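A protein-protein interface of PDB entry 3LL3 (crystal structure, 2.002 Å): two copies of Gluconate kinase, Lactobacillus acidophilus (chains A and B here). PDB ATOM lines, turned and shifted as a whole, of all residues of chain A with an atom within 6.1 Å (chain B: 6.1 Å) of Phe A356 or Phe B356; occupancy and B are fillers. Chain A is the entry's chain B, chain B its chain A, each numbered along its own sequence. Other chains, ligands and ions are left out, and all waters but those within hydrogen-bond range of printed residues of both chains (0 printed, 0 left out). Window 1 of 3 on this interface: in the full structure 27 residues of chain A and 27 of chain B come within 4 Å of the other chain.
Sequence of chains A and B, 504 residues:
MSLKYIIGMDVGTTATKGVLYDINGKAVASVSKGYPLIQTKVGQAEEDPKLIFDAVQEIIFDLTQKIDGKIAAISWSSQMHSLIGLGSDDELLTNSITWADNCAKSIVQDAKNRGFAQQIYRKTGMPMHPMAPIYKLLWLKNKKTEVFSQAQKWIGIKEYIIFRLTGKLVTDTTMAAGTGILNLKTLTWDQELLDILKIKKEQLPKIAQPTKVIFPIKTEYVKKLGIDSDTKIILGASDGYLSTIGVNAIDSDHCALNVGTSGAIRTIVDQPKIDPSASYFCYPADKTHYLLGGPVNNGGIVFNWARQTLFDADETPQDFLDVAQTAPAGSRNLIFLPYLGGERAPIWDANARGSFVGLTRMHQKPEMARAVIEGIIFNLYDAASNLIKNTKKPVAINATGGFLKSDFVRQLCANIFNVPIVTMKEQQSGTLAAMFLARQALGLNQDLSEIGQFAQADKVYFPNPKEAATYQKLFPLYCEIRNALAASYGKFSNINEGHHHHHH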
ATOM      1  N   TRP A 305      34.911 -18.168 -20.750  1.00  0.00           N
ATOM      2  CA  TRP A 305      33.715 -18.989 -20.584  1.00  0.00           C
ATOM      3  C   TRP A 305      32.544 -18.176 -20.025  1.00  0.00           C
ATOM      4  O   TRP A 305      31.436 -18.196 -20.580  1.00  0.00           O
ATOM      5  CB  TRP A 305      33.984 -20.166 -19.659  1.00  0.00           C
ATOM      6  CG  TRP A 305      32.730 -20.870 -19.296  1.00  0.00           C
ATOM      7  CD1 TRP A 305      32.053 -21.775 -20.058  1.00  0.00           C
ATOM      8  CD2 TRP A 305      31.978 -20.719 -18.087  1.00  0.00           C
ATOM      9  NE1 TRP A 305      30.928 -22.208 -19.388  1.00  0.00           N
ATOM     10  CE2 TRP A 305      30.856 -21.569 -18.182  1.00  0.00           C
ATOM     11  CE3 TRP A 305      32.148 -19.954 -16.929  1.00  0.00           C
ATOM     12  CZ2 TRP A 305      29.908 -21.673 -17.164  1.00  0.00           C
ATOM     13  CZ3 TRP A 305      31.210 -20.052 -15.925  1.00  0.00           C
ATOM     14  CH2 TRP A 305      30.098 -20.908 -16.047  1.00  0.00           C
ATOM     15  N   LEU A 310      27.495 -16.428 -19.254  1.00  0.00           N
ATOM     16  CA  LEU A 310      26.688 -15.550 -18.419  1.00  0.00           C
ATOM     17  C   LEU A 310      25.986 -14.492 -19.276  1.00  0.00           C
ATOM     18  O   LEU A 310      24.889 -14.069 -18.953  1.00  0.00           O
ATOM     19  CB  LEU A 310      27.559 -14.905 -17.329  1.00  0.00           C
ATOM     20  CG  LEU A 310      27.507 -15.406 -15.876  1.00  0.00           C
ATOM     21  CD1 LEU A 310      27.067 -16.871 -15.716  1.00  0.00           C
ATOM     22  CD2 LEU A 310      28.844 -15.154 -15.184  1.00  0.00           C
ATOM     23  N   LEU A 334      28.884 -14.100  -2.572  1.00  0.00           N
ATOM     24  CA  LEU A 334      28.789 -15.190  -3.546  1.00  0.00           C
ATOM     25  C   LEU A 334      30.185 -15.763  -3.814  1.00  0.00           C
ATOM     26  O   LEU A 334      31.114 -15.018  -4.096  1.00  0.00           O
ATOM     27  CB  LEU A 334      28.154 -14.694  -4.852  1.00  0.00           C
ATOM     28  CG  LEU A 334      27.992 -15.700  -5.996  1.00  0.00           C
ATOM     29  CD1 LEU A 334      27.120 -16.878  -5.568  1.00  0.00           C
ATOM     30  CD2 LEU A 334      27.395 -14.991  -7.202  1.00  0.00           C
ATOM     31  N   ILE A 335      30.331 -17.080  -3.710  1.00  0.00           N
ATOM     32  CA  ILE A 335      31.599 -17.754  -3.993  1.00  0.00           C
ATOM     33  C   ILE A 335      31.551 -18.475  -5.342  1.00  0.00           C
ATOM     34  O   ILE A 335      30.580 -19.206  -5.631  1.00  0.00           O
ATOM     35  CB  ILE A 335      31.917 -18.792  -2.924  1.00  0.00           C
ATOM     36  CG1 ILE A 335      32.145 -18.114  -1.562  1.00  0.00           C
ATOM     37  CG2 ILE A 335      33.117 -19.622  -3.342  1.00  0.00           C
ATOM     38  CD1 ILE A 335      33.220 -17.029  -1.593  1.00  0.00           C
ATOM     39  N   PHE A 336      32.582 -18.255  -6.164  1.00  0.00           N
ATOM     40  CA  PHE A 336      32.765 -19.003  -7.393  1.00  0.00           C
ATOM     41  C   PHE A 336      34.058 -19.785  -7.307  1.00  0.00           C
ATOM     42  O   PHE A 336      35.131 -19.182  -7.310  1.00  0.00           O
ATOM     43  CB  PHE A 336      32.793 -18.056  -8.606  1.00  0.00           C
ATOM     44  CG  PHE A 336      33.048 -18.744  -9.919  1.00  0.00           C
ATOM     45  CD1 PHE A 336      32.060 -19.497 -10.529  1.00  0.00           C
ATOM     46  CD2 PHE A 336      34.273 -18.603 -10.568  1.00  0.00           C
ATOM     47  CE1 PHE A 336      32.294 -20.116 -11.762  1.00  0.00           C
ATOM     48  CE2 PHE A 336      34.508 -19.207 -11.797  1.00  0.00           C
ATOM     49  CZ  PHE A 336      33.549 -19.965 -12.388  1.00  0.00           C
ATOM     50  N   LEU A 337      33.972 -21.111  -7.198  1.00  0.00           N
ATOM     51  CA  LEU A 337      35.170 -21.955  -7.316  1.00  0.00           C
ATOM     52  C   LEU A 337      35.405 -22.158  -8.821  1.00  0.00           C
ATOM     53  O   LEU A 337      34.550 -22.713  -9.524  1.00  0.00           O
ATOM     54  CB  LEU A 337      35.002 -23.293  -6.580  1.00  0.00           C
ATOM     55  CG  LEU A 337      34.649 -23.213  -5.083  1.00  0.00           C
ATOM     56  CD1 LEU A 337      34.293 -24.591  -4.483  1.00  0.00           C
ATOM     57  CD2 LEU A 337      35.767 -22.551  -4.274  1.00  0.00           C
ATOM     58  N   GLY A 354      33.678 -26.426 -11.579  1.00  0.00           N
ATOM     59  CA  GLY A 354      33.397 -25.131 -10.973  1.00  0.00           C
ATOM     60  C   GLY A 354      32.057 -25.063 -10.245  1.00  0.00           C
ATOM     61  O   GLY A 354      31.172 -25.905 -10.450  1.00  0.00           O
ATOM     62  N   SER A 355      31.894 -24.056  -9.395  1.00  0.00           N
ATOM     63  CA  SER A 355      30.636 -23.896  -8.659  1.00  0.00           C
ATOM     64  C   SER A 355      30.364 -22.440  -8.349  1.00  0.00           C
ATOM     65  O   SER A 355      31.289 -21.671  -8.107  1.00  0.00           O
ATOM     66  CB  SER A 355      30.706 -24.654  -7.327  1.00  0.00           C
ATOM     67  OG  SER A 355      30.945 -26.041  -7.522  1.00  0.00           O
ATOM     68  N   PHE A 356      29.092 -22.059  -8.354  1.00  0.00           N
ATOM     69  CA  PHE A 356      28.667 -20.853  -7.652  1.00  0.00           C
ATOM     70  C   PHE A 356      27.978 -21.348  -6.390  1.00  0.00           C
ATOM     71  O   PHE A 356      27.049 -22.154  -6.489  1.00  0.00           O
ATOM     72  CB  PHE A 356      27.643 -20.084  -8.480  1.00  0.00           C
ATOM     73  CG  PHE A 356      28.209 -19.358  -9.672  1.00  0.00           C
ATOM     74  CD1 PHE A 356      28.705 -18.069  -9.547  1.00  0.00           C
ATOM     75  CD2 PHE A 356      28.171 -19.929 -10.925  1.00  0.00           C
ATOM     76  CE1 PHE A 356      29.188 -17.377 -10.661  1.00  0.00           C
ATOM     77  CE2 PHE A 356      28.649 -19.249 -12.046  1.00  0.00           C
ATOM     78  CZ  PHE A 356      29.158 -17.970 -11.911  1.00  0.00           C
ATOM     79  N   VAL A 357      28.425 -20.890  -5.220  1.00  0.00           N
ATOM     80  CA  VAL A 357      27.798 -21.247  -3.946  1.00  0.00           C
ATOM     81  C   VAL A 357      27.438 -19.989  -3.156  1.00  0.00           C
ATOM     82  O   VAL A 357      28.273 -19.081  -3.012  1.00  0.00           O
ATOM     83  CB  VAL A 357      28.712 -22.154  -3.089  1.00  0.00           C
ATOM     84  CG1 VAL A 357      28.039 -22.527  -1.776  1.00  0.00           C
ATOM     85  CG2 VAL A 357      29.056 -23.417  -3.859  1.00  0.00           C
ATOM     86  N   GLY A 358      26.192 -19.929  -2.678  1.00  0.00           N
ATOM     87  CA  GLY A 358      25.718 -18.817  -1.865  1.00  0.00           C
ATOM     88  C   GLY A 358      24.711 -17.923  -2.550  1.00  0.00           C
ATOM     89  O   GLY A 358      24.587 -16.760  -2.214  1.00  0.00           O
ATOM     90  N   LEU A 359      23.979 -18.462  -3.523  1.00  0.00           N
ATOM     91  CA  LEU A 359      23.021 -17.668  -4.287  1.00  0.00           C
ATOM     92  C   LEU A 359      21.748 -17.286  -3.522  1.00  0.00           C
ATOM     93  O   LEU A 359      21.155 -18.072  -2.791  1.00  0.00           O
ATOM     94  CB  LEU A 359      22.616 -18.375  -5.585  1.00  0.00           C
ATOM     95  CG  LEU A 359      23.667 -18.545  -6.684  1.00  0.00           C
ATOM     96  CD1 LEU A 359      23.198 -19.571  -7.712  1.00  0.00           C
ATOM     97  CD2 LEU A 359      23.970 -17.219  -7.358  1.00  0.00           C
ATOM     98  N   GLU A 367      26.554  -9.511  -9.607  1.00  0.00           N
ATOM     99  CA  GLU A 367      27.172 -10.330  -8.572  1.00  0.00           C
ATOM    100  C   GLU A 367      27.810 -11.612  -9.127  1.00  0.00           C
ATOM    101  O   GLU A 367      28.868 -12.047  -8.657  1.00  0.00           O
ATOM    102  CB  GLU A 367      26.146 -10.677  -7.493  1.00  0.00           C
ATOM    103  CG  GLU A 367      25.886  -9.563  -6.480  1.00  0.00           C
ATOM    104  CD  GLU A 367      25.120  -8.365  -7.039  1.00  0.00           C
ATOM    105  OE1 GLU A 367      24.407  -8.503  -8.058  1.00  0.00           O
ATOM    106  OE2 GLU A 367      25.220  -7.279  -6.430  1.00  0.00           O
ATOM    107  N   MET A 368      27.159 -12.236 -10.105  1.00  0.00           N
ATOM    108  CA  MET A 368      27.679 -13.477 -10.666  1.00  0.00           C
ATOM    109  C   MET A 368      28.907 -13.183 -11.529  1.00  0.00           C
ATOM    110  O   MET A 368      29.918 -13.872 -11.421  1.00  0.00           O
ATOM    111  CB  MET A 368      26.615 -14.218 -11.472  1.00  0.00           C
ATOM    112  CG  MET A 368      25.437 -14.709 -10.601  1.00  0.00           C
ATOM    113  SD  MET A 368      24.224 -15.875 -11.591  1.00  0.00           S
ATOM    114  CE  MET A 368      25.334 -17.516 -11.598  1.00  0.00           C
ATOM    115  N   ALA A 369      28.814 -12.163 -12.380  1.00  0.00           N
ATOM    116  CA  ALA A 369      29.967 -11.730 -13.168  1.00  0.00           C
ATOM    117  C   ALA A 369      31.145 -11.401 -12.244  1.00  0.00           C
ATOM    118  O   ALA A 369      32.239 -11.926 -12.444  1.00  0.00           O
ATOM    119  CB  ALA A 369      29.615 -10.543 -14.058  1.00  0.00           C
ATOM    120  N   ALA A 371      31.739 -12.346  -9.126  1.00  0.00           N
ATOM    121  CA  ALA A 371      32.196 -13.511  -8.367  1.00  0.00           C
ATOM    122  C   ALA A 371      33.123 -14.392  -9.186  1.00  0.00           C
ATOM    123  O   ALA A 371      34.022 -15.008  -8.637  1.00  0.00           O
ATOM    124  CB  ALA A 371      31.010 -14.342  -7.852  1.00  0.00           C
ATOM    125  N   VAL A 372      32.882 -14.482 -10.490  1.00  0.00           N
ATOM    126  CA  VAL A 372      33.774 -15.223 -11.376  1.00  0.00           C
ATOM    127  C   VAL A 372      35.194 -14.627 -11.313  1.00  0.00           C
ATOM    128  O   VAL A 372      36.191 -15.350 -11.139  1.00  0.00           O
ATOM    129  CB  VAL A 372      33.265 -15.212 -12.850  1.00  0.00           C
ATOM    130  CG1 VAL A 372      34.389 -15.573 -13.816  1.00  0.00           C
ATOM    131  CG2 VAL A 372      32.052 -16.150 -13.037  1.00  0.00           C
ATOM    132  N   TRP B 305      13.701 -15.714 -10.831  1.00  0.00           N
ATOM    133  CA  TRP B 305      15.054 -15.202 -10.593  1.00  0.00           C
ATOM    134  C   TRP B 305      16.017 -15.611 -11.710  1.00  0.00           C
ATOM    135  O   TRP B 305      16.776 -14.781 -12.210  1.00  0.00           O
ATOM    136  CB  TRP B 305      15.607 -15.648  -9.234  1.00  0.00           C
ATOM    137  CG  TRP B 305      17.084 -15.391  -9.101  1.00  0.00           C
ATOM    138  CD1 TRP B 305      17.687 -14.248  -8.638  1.00  0.00           C
ATOM    139  CD2 TRP B 305      18.150 -16.294  -9.443  1.00  0.00           C
ATOM    140  NE1 TRP B 305      19.060 -14.393  -8.662  1.00  0.00           N
ATOM    141  CE2 TRP B 305      19.369 -15.634  -9.156  1.00  0.00           C
ATOM    142  CE3 TRP B 305      18.192 -17.598  -9.954  1.00  0.00           C
ATOM    143  CZ2 TRP B 305      20.614 -16.233  -9.371  1.00  0.00           C
ATOM    144  CZ3 TRP B 305      19.434 -18.191 -10.170  1.00  0.00           C
ATOM    145  CH2 TRP B 305      20.631 -17.505  -9.879  1.00  0.00           C
ATOM    146  N   LEU B 310      19.973 -15.046 -15.452  1.00  0.00           N
ATOM    147  CA  LEU B 310      20.749 -15.766 -16.451  1.00  0.00           C
ATOM    148  C   LEU B 310      20.651 -15.056 -17.785  1.00  0.00           C
ATOM    149  O   LEU B 310      21.585 -15.108 -18.570  1.00  0.00           O
ATOM    150  CB  LEU B 310      20.301 -17.226 -16.596  1.00  0.00           C
ATOM    151  CG  LEU B 310      20.814 -18.187 -15.522  1.00  0.00           C
ATOM    152  CD1 LEU B 310      20.492 -17.603 -14.184  1.00  0.00           C
ATOM    153  CD2 LEU B 310      20.209 -19.570 -15.626  1.00  0.00           C
ATOM    154  N   LEU B 334      25.100 -31.097 -14.454  1.00  0.00           N
ATOM    155  CA  LEU B 334      25.169 -29.880 -13.669  1.00  0.00           C
ATOM    156  C   LEU B 334      24.078 -29.920 -12.586  1.00  0.00           C
ATOM    157  O   LEU B 334      22.918 -30.165 -12.885  1.00  0.00           O
ATOM    158  CB  LEU B 334      25.028 -28.655 -14.568  1.00  0.00           C
ATOM    159  CG  LEU B 334      25.022 -27.308 -13.839  1.00  0.00           C
ATOM    160  CD1 LEU B 334      26.335 -27.107 -13.066  1.00  0.00           C
ATOM    161  CD2 LEU B 334      24.781 -26.186 -14.823  1.00  0.00           C
ATOM    162  N   ILE B 335      24.461 -29.695 -11.331  1.00  0.00           N
ATOM    163  CA  ILE B 335      23.508 -29.648 -10.227  1.00  0.00           C
ATOM    164  C   ILE B 335      23.182 -28.207  -9.809  1.00  0.00           C
ATOM    165  O   ILE B 335      24.088 -27.382  -9.618  1.00  0.00           O
ATOM    166  CB  ILE B 335      24.030 -30.401  -8.993  1.00  0.00           C
ATOM    167  CG1 ILE B 335      24.113 -31.901  -9.282  1.00  0.00           C
ATOM    168  CG2 ILE B 335      23.125 -30.118  -7.765  1.00  0.00           C
ATOM    169  CD1 ILE B 335      22.823 -32.490  -9.827  1.00  0.00           C
ATOM    170  N   PHE B 336      21.890 -27.917  -9.671  1.00  0.00           N
ATOM    171  CA  PHE B 336      21.430 -26.647  -9.132  1.00  0.00           C
ATOM    172  C   PHE B 336      20.646 -26.906  -7.856  1.00  0.00           C
ATOM    173  O   PHE B 336      19.550 -27.481  -7.909  1.00  0.00           O
ATOM    174  CB  PHE B 336      20.547 -25.899 -10.133  1.00  0.00           C
ATOM    175  CG  PHE B 336      20.039 -24.569  -9.623  1.00  0.00           C
ATOM    176  CD1 PHE B 336      20.898 -23.481  -9.479  1.00  0.00           C
ATOM    177  CD2 PHE B 336      18.704 -24.396  -9.299  1.00  0.00           C
ATOM    178  CE1 PHE B 336      20.425 -22.248  -9.019  1.00  0.00           C
ATOM    179  CE2 PHE B 336      18.229 -23.181  -8.839  1.00  0.00           C
ATOM    180  CZ  PHE B 336      19.080 -22.106  -8.692  1.00  0.00           C
ATOM    181  N   LEU B 337      21.206 -26.509  -6.715  1.00  0.00           N
ATOM    182  CA  LEU B 337      20.433 -26.534  -5.468  1.00  0.00           C
ATOM    183  C   LEU B 337      19.632 -25.228  -5.409  1.00  0.00           C
ATOM    184  O   LEU B 337      20.208 -24.146  -5.411  1.00  0.00           O
ATOM    185  CB  LEU B 337      21.343 -26.690  -4.241  1.00  0.00           C
ATOM    186  CG  LEU B 337      22.286 -27.904  -4.188  1.00  0.00           C
ATOM    187  CD1 LEU B 337      23.145 -27.913  -2.907  1.00  0.00           C
ATOM    188  CD2 LEU B 337      21.493 -29.195  -4.298  1.00  0.00           C
ATOM    189  N   GLY B 354      21.292 -20.905  -2.611  1.00  0.00           N
ATOM    190  CA  GLY B 354      21.351 -21.709  -3.826  1.00  0.00           C
ATOM    191  C   GLY B 354      22.769 -21.923  -4.347  1.00  0.00           C
ATOM    192  O   GLY B 354      23.661 -21.148  -4.001  1.00  0.00           O
ATOM    193  N   SER B 355      22.972 -22.964  -5.162  1.00  0.00           N
ATOM    194  CA  SER B 355      24.282 -23.275  -5.743  1.00  0.00           C
ATOM    195  C   SER B 355      24.143 -23.895  -7.139  1.00  0.00           C
ATOM    196  O   SER B 355      23.188 -24.636  -7.397  1.00  0.00           O
ATOM    197  CB  SER B 355      25.050 -24.280  -4.865  1.00  0.00           C
ATOM    198  OG  SER B 355      25.219 -23.802  -3.539  1.00  0.00           O
ATOM    199  N   PHE B 356      25.090 -23.591  -8.026  1.00  0.00           N
ATOM    200  CA  PHE B 356      25.336 -24.413  -9.206  1.00  0.00           C
ATOM    201  C   PHE B 356      26.587 -25.198  -8.900  1.00  0.00           C
ATOM    202  O   PHE B 356      27.620 -24.589  -8.649  1.00  0.00           O
ATOM    203  CB  PHE B 356      25.629 -23.561 -10.451  1.00  0.00           C
ATOM    204  CG  PHE B 356      24.409 -22.922 -11.073  1.00  0.00           C
ATOM    205  CD1 PHE B 356      23.616 -23.634 -11.966  1.00  0.00           C
ATOM    206  CD2 PHE B 356      24.081 -21.601 -10.791  1.00  0.00           C
ATOM    207  CE1 PHE B 356      22.506 -23.047 -12.563  1.00  0.00           C
ATOM    208  CE2 PHE B 356      22.962 -20.998 -11.373  1.00  0.00           C
ATOM    209  CZ  PHE B 356      22.161 -21.723 -12.245  1.00  0.00           C
ATOM    210  N   VAL B 357      26.536 -26.524  -8.948  1.00  0.00           N
ATOM    211  CA  VAL B 357      27.755 -27.321  -8.746  1.00  0.00           C
ATOM    212  C   VAL B 357      27.994 -28.328  -9.871  1.00  0.00           C
ATOM    213  O   VAL B 357      27.096 -29.088 -10.234  1.00  0.00           O
ATOM    214  CB  VAL B 357      27.758 -28.061  -7.374  1.00  0.00           C
ATOM    215  CG1 VAL B 357      29.062 -28.870  -7.185  1.00  0.00           C
ATOM    216  CG2 VAL B 357      27.569 -27.081  -6.225  1.00  0.00           C
ATOM    217  N   GLY B 358      29.214 -28.339 -10.417  1.00  0.00           N
ATOM    218  CA  GLY B 358      29.570 -29.270 -11.474  1.00  0.00           C
ATOM    219  C   GLY B 358      29.868 -28.632 -12.820  1.00  0.00           C
ATOM    220  O   GLY B 358      29.744 -29.268 -13.852  1.00  0.00           O
ATOM    221  N   LEU B 359      30.251 -27.363 -12.815  1.00  0.00           N
ATOM    222  CA  LEU B 359      30.461 -26.629 -14.056  1.00  0.00           C
ATOM    223  C   LEU B 359      31.775 -27.011 -14.764  1.00  0.00           C
ATOM    224  O   LEU B 359      32.780 -27.355 -14.134  1.00  0.00           O
ATOM    225  CB  LEU B 359      30.440 -25.120 -13.816  1.00  0.00           C
ATOM    226  CG  LEU B 359      29.150 -24.404 -13.417  1.00  0.00           C
ATOM    227  CD1 LEU B 359      29.489 -23.051 -12.810  1.00  0.00           C
ATOM    228  CD2 LEU B 359      28.222 -24.237 -14.627  1.00  0.00           C
ATOM    229  N   GLU B 367      22.534 -25.398 -20.556  1.00  0.00           N
ATOM    230  CA  GLU B 367      22.792 -26.275 -19.417  1.00  0.00           C
ATOM    231  C   GLU B 367      22.459 -25.605 -18.075  1.00  0.00           C
ATOM    232  O   GLU B 367      21.931 -26.254 -17.176  1.00  0.00           O
ATOM    233  CB  GLU B 367      24.256 -26.732 -19.401  1.00  0.00           C
ATOM    234  CG  GLU B 367      24.602 -27.860 -20.388  1.00  0.00           C
ATOM    235  CD  GLU B 367      24.549 -27.422 -21.846  1.00  0.00           C
ATOM    236  OE1 GLU B 367      24.783 -26.230 -22.155  1.00  0.00           O
ATOM    237  OE2 GLU B 367      24.270 -28.285 -22.688  1.00  0.00           O
ATOM    238  N   MET B 368      22.772 -24.319 -17.930  1.00  0.00           N
ATOM    239  CA  MET B 368      22.460 -23.638 -16.675  1.00  0.00           C
ATOM    240  C   MET B 368      20.976 -23.410 -16.530  1.00  0.00           C
ATOM    241  O   MET B 368      20.440 -23.605 -15.450  1.00  0.00           O
ATOM    242  CB  MET B 368      23.219 -22.331 -16.521  1.00  0.00           C
ATOM    243  CG  MET B 368      24.741 -22.594 -16.500  1.00  0.00           C
ATOM    244  SD  MET B 368      25.758 -20.994 -16.122  1.00  0.00           S
ATOM    245  CE  MET B 368      25.412 -20.828 -14.187  1.00  0.00           C
ATOM    246  N   ALA B 369      20.324 -23.020 -17.629  1.00  0.00           N
ATOM    247  CA  ALA B 369      18.881 -22.798 -17.639  1.00  0.00           C
ATOM    248  C   ALA B 369      18.162 -24.072 -17.253  1.00  0.00           C
ATOM    249  O   ALA B 369      17.276 -24.060 -16.405  1.00  0.00           O
ATOM    250  CB  ALA B 369      18.405 -22.328 -19.025  1.00  0.00           C
ATOM    251  N   ALA B 371      19.380 -26.773 -15.749  1.00  0.00           N
ATOM    252  CA  ALA B 371      19.735 -27.209 -14.405  1.00  0.00           C
ATOM    253  C   ALA B 371      18.853 -26.530 -13.376  1.00  0.00           C
ATOM    254  O   ALA B 371      18.519 -27.138 -12.364  1.00  0.00           O
ATOM    255  CB  ALA B 371      21.226 -26.932 -14.091  1.00  0.00           C
ATOM    256  N   VAL B 372      18.496 -25.270 -13.617  1.00  0.00           N
ATOM    257  CA  VAL B 372      17.630 -24.548 -12.688  1.00  0.00           C
ATOM    258  C   VAL B 372      16.273 -25.251 -12.614  1.00  0.00           C
ATOM    259  O   VAL B 372      15.772 -25.553 -11.527  1.00  0.00           O
ATOM    260  CB  VAL B 372      17.420 -23.075 -13.102  1.00  0.00           C
ATOM    261  CG1 VAL B 372      16.259 -22.458 -12.309  1.00  0.00           C
ATOM    262  CG2 VAL B 372      18.720 -22.255 -12.930  1.00  0.00           C
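O of Gly B354 is in hydrogen-bond range of N of Gly A358 (3.1 Å).
O of Gly B354 sits at hydrogen-bond distance from N of Leu A359, at 2.7 Å.
N of Phe B356 lies within hydrogen-bond range of O of Phe A356 (2.9 Å).
The backbone NH (N) of Gly B358 sits at hydrogen-bond distance from the backbone carbonyl oxygen (O) of Gly A354 (3.1 Å).
O of Leu B359 sits at hydrogen-bond distance from N of Gly A354 (2.9 Å).
The backbone carbonyl oxygen of Leu A310 lies close to the backbone carbonyl oxygen of Leu B310, at 3.5 Å.
The backbone carbonyl oxygen (O) of Ile B335 is in hydrogen-bond range of the backbone NH (N) of Val B357 (2.7 Å).
The backbone NH (N) of Leu B337 sits at hydrogen-bond distance from the backbone carbonyl oxygen (O) of Ser B355 (2.8 Å).
O of Ile A335 sits at hydrogen-bond distance from N of Val A357 (2.8 Å).
The backbone carbonyl oxygen (O) of Ser A355 sits at hydrogen-bond distance from the backbone NH (N) of Leu A337 (2.9 Å).
Among the printed residues, pairs that only touch across the chains: Phe A356 with Ser B355 (3.1 Å), Ser A355 with Phe B356 (3.1 Å), Ser A355 with Val B357 (3.4 Å), Val A357 with Ser B355 (3.6 Å), Leu A359 with Phe B356 (3.8 Å), Phe A356 with Leu B359 (3.9 Å), Trp A305 with Leu B359 (3.9 Å) and Leu A359 with Trp B305 (3.9 Å).
Of the printed residues of chain B, Trp A305 touches Leu B359.
Printed residues of chain B within 4 Å of Gly A358: Gly B354.
Printed residues of chain B within 4 Å of Leu A359: Trp B305 (3.9 Å), Gly B354 (2.7 Å) and Phe B356 (3.8 Å).
Glu A367 touches none of the printed residues of chain B.
Leu B337 touches none of the printed residues of chain A.
Phe B356 touches just these residues of chain A: Ser A355, Phe A356 and Leu A359.
The nearest printed residue of chain A that does not touch Phe B356 is Gly A354 (4.2 Å).
The nearest printed residue of chain B that does not touch Val A357 is Gly B354 (4.04 Å).
Hydrophobic or aromatic side chains of chain B that line the printed part of chain A: Trp B305, Phe B356, Val B357 and Leu B359.
Of the 17 printed residues of chain A, 8 touch a printed residue of chain B.
Printed residues of chain A that touch a printed residue of chain B: Trp A305, Leu A310, Gly A354, Ser A355, Phe A356, Val A357, Gly A358 and Leu A359.
Hydrophobic or aromatic side chains of chain A within 4 Å of the printed part of chain B: Trp A305, Phe A356, Val A357 and Leu A359.
Among the printed residues, 14 pairs touch across the chains.
Among the printed residues, no Asp or Glu carboxylate lies within 4 Å of a Lys or Arg side-chain nitrogen of the other chain.
Gly A354 touches Gly B358, and with the chains exchanged Gly A358 touches Gly B354.
Gly A354 touches Leu B359, and with the chains exchanged Leu A359 touches Gly B354.
Ser A355 touches Val B357, and with the chains exchanged Val A357 touches Ser B355.
Phe A356 touches its own counterpart, Phe B356.
17 positions are printed for both chains.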
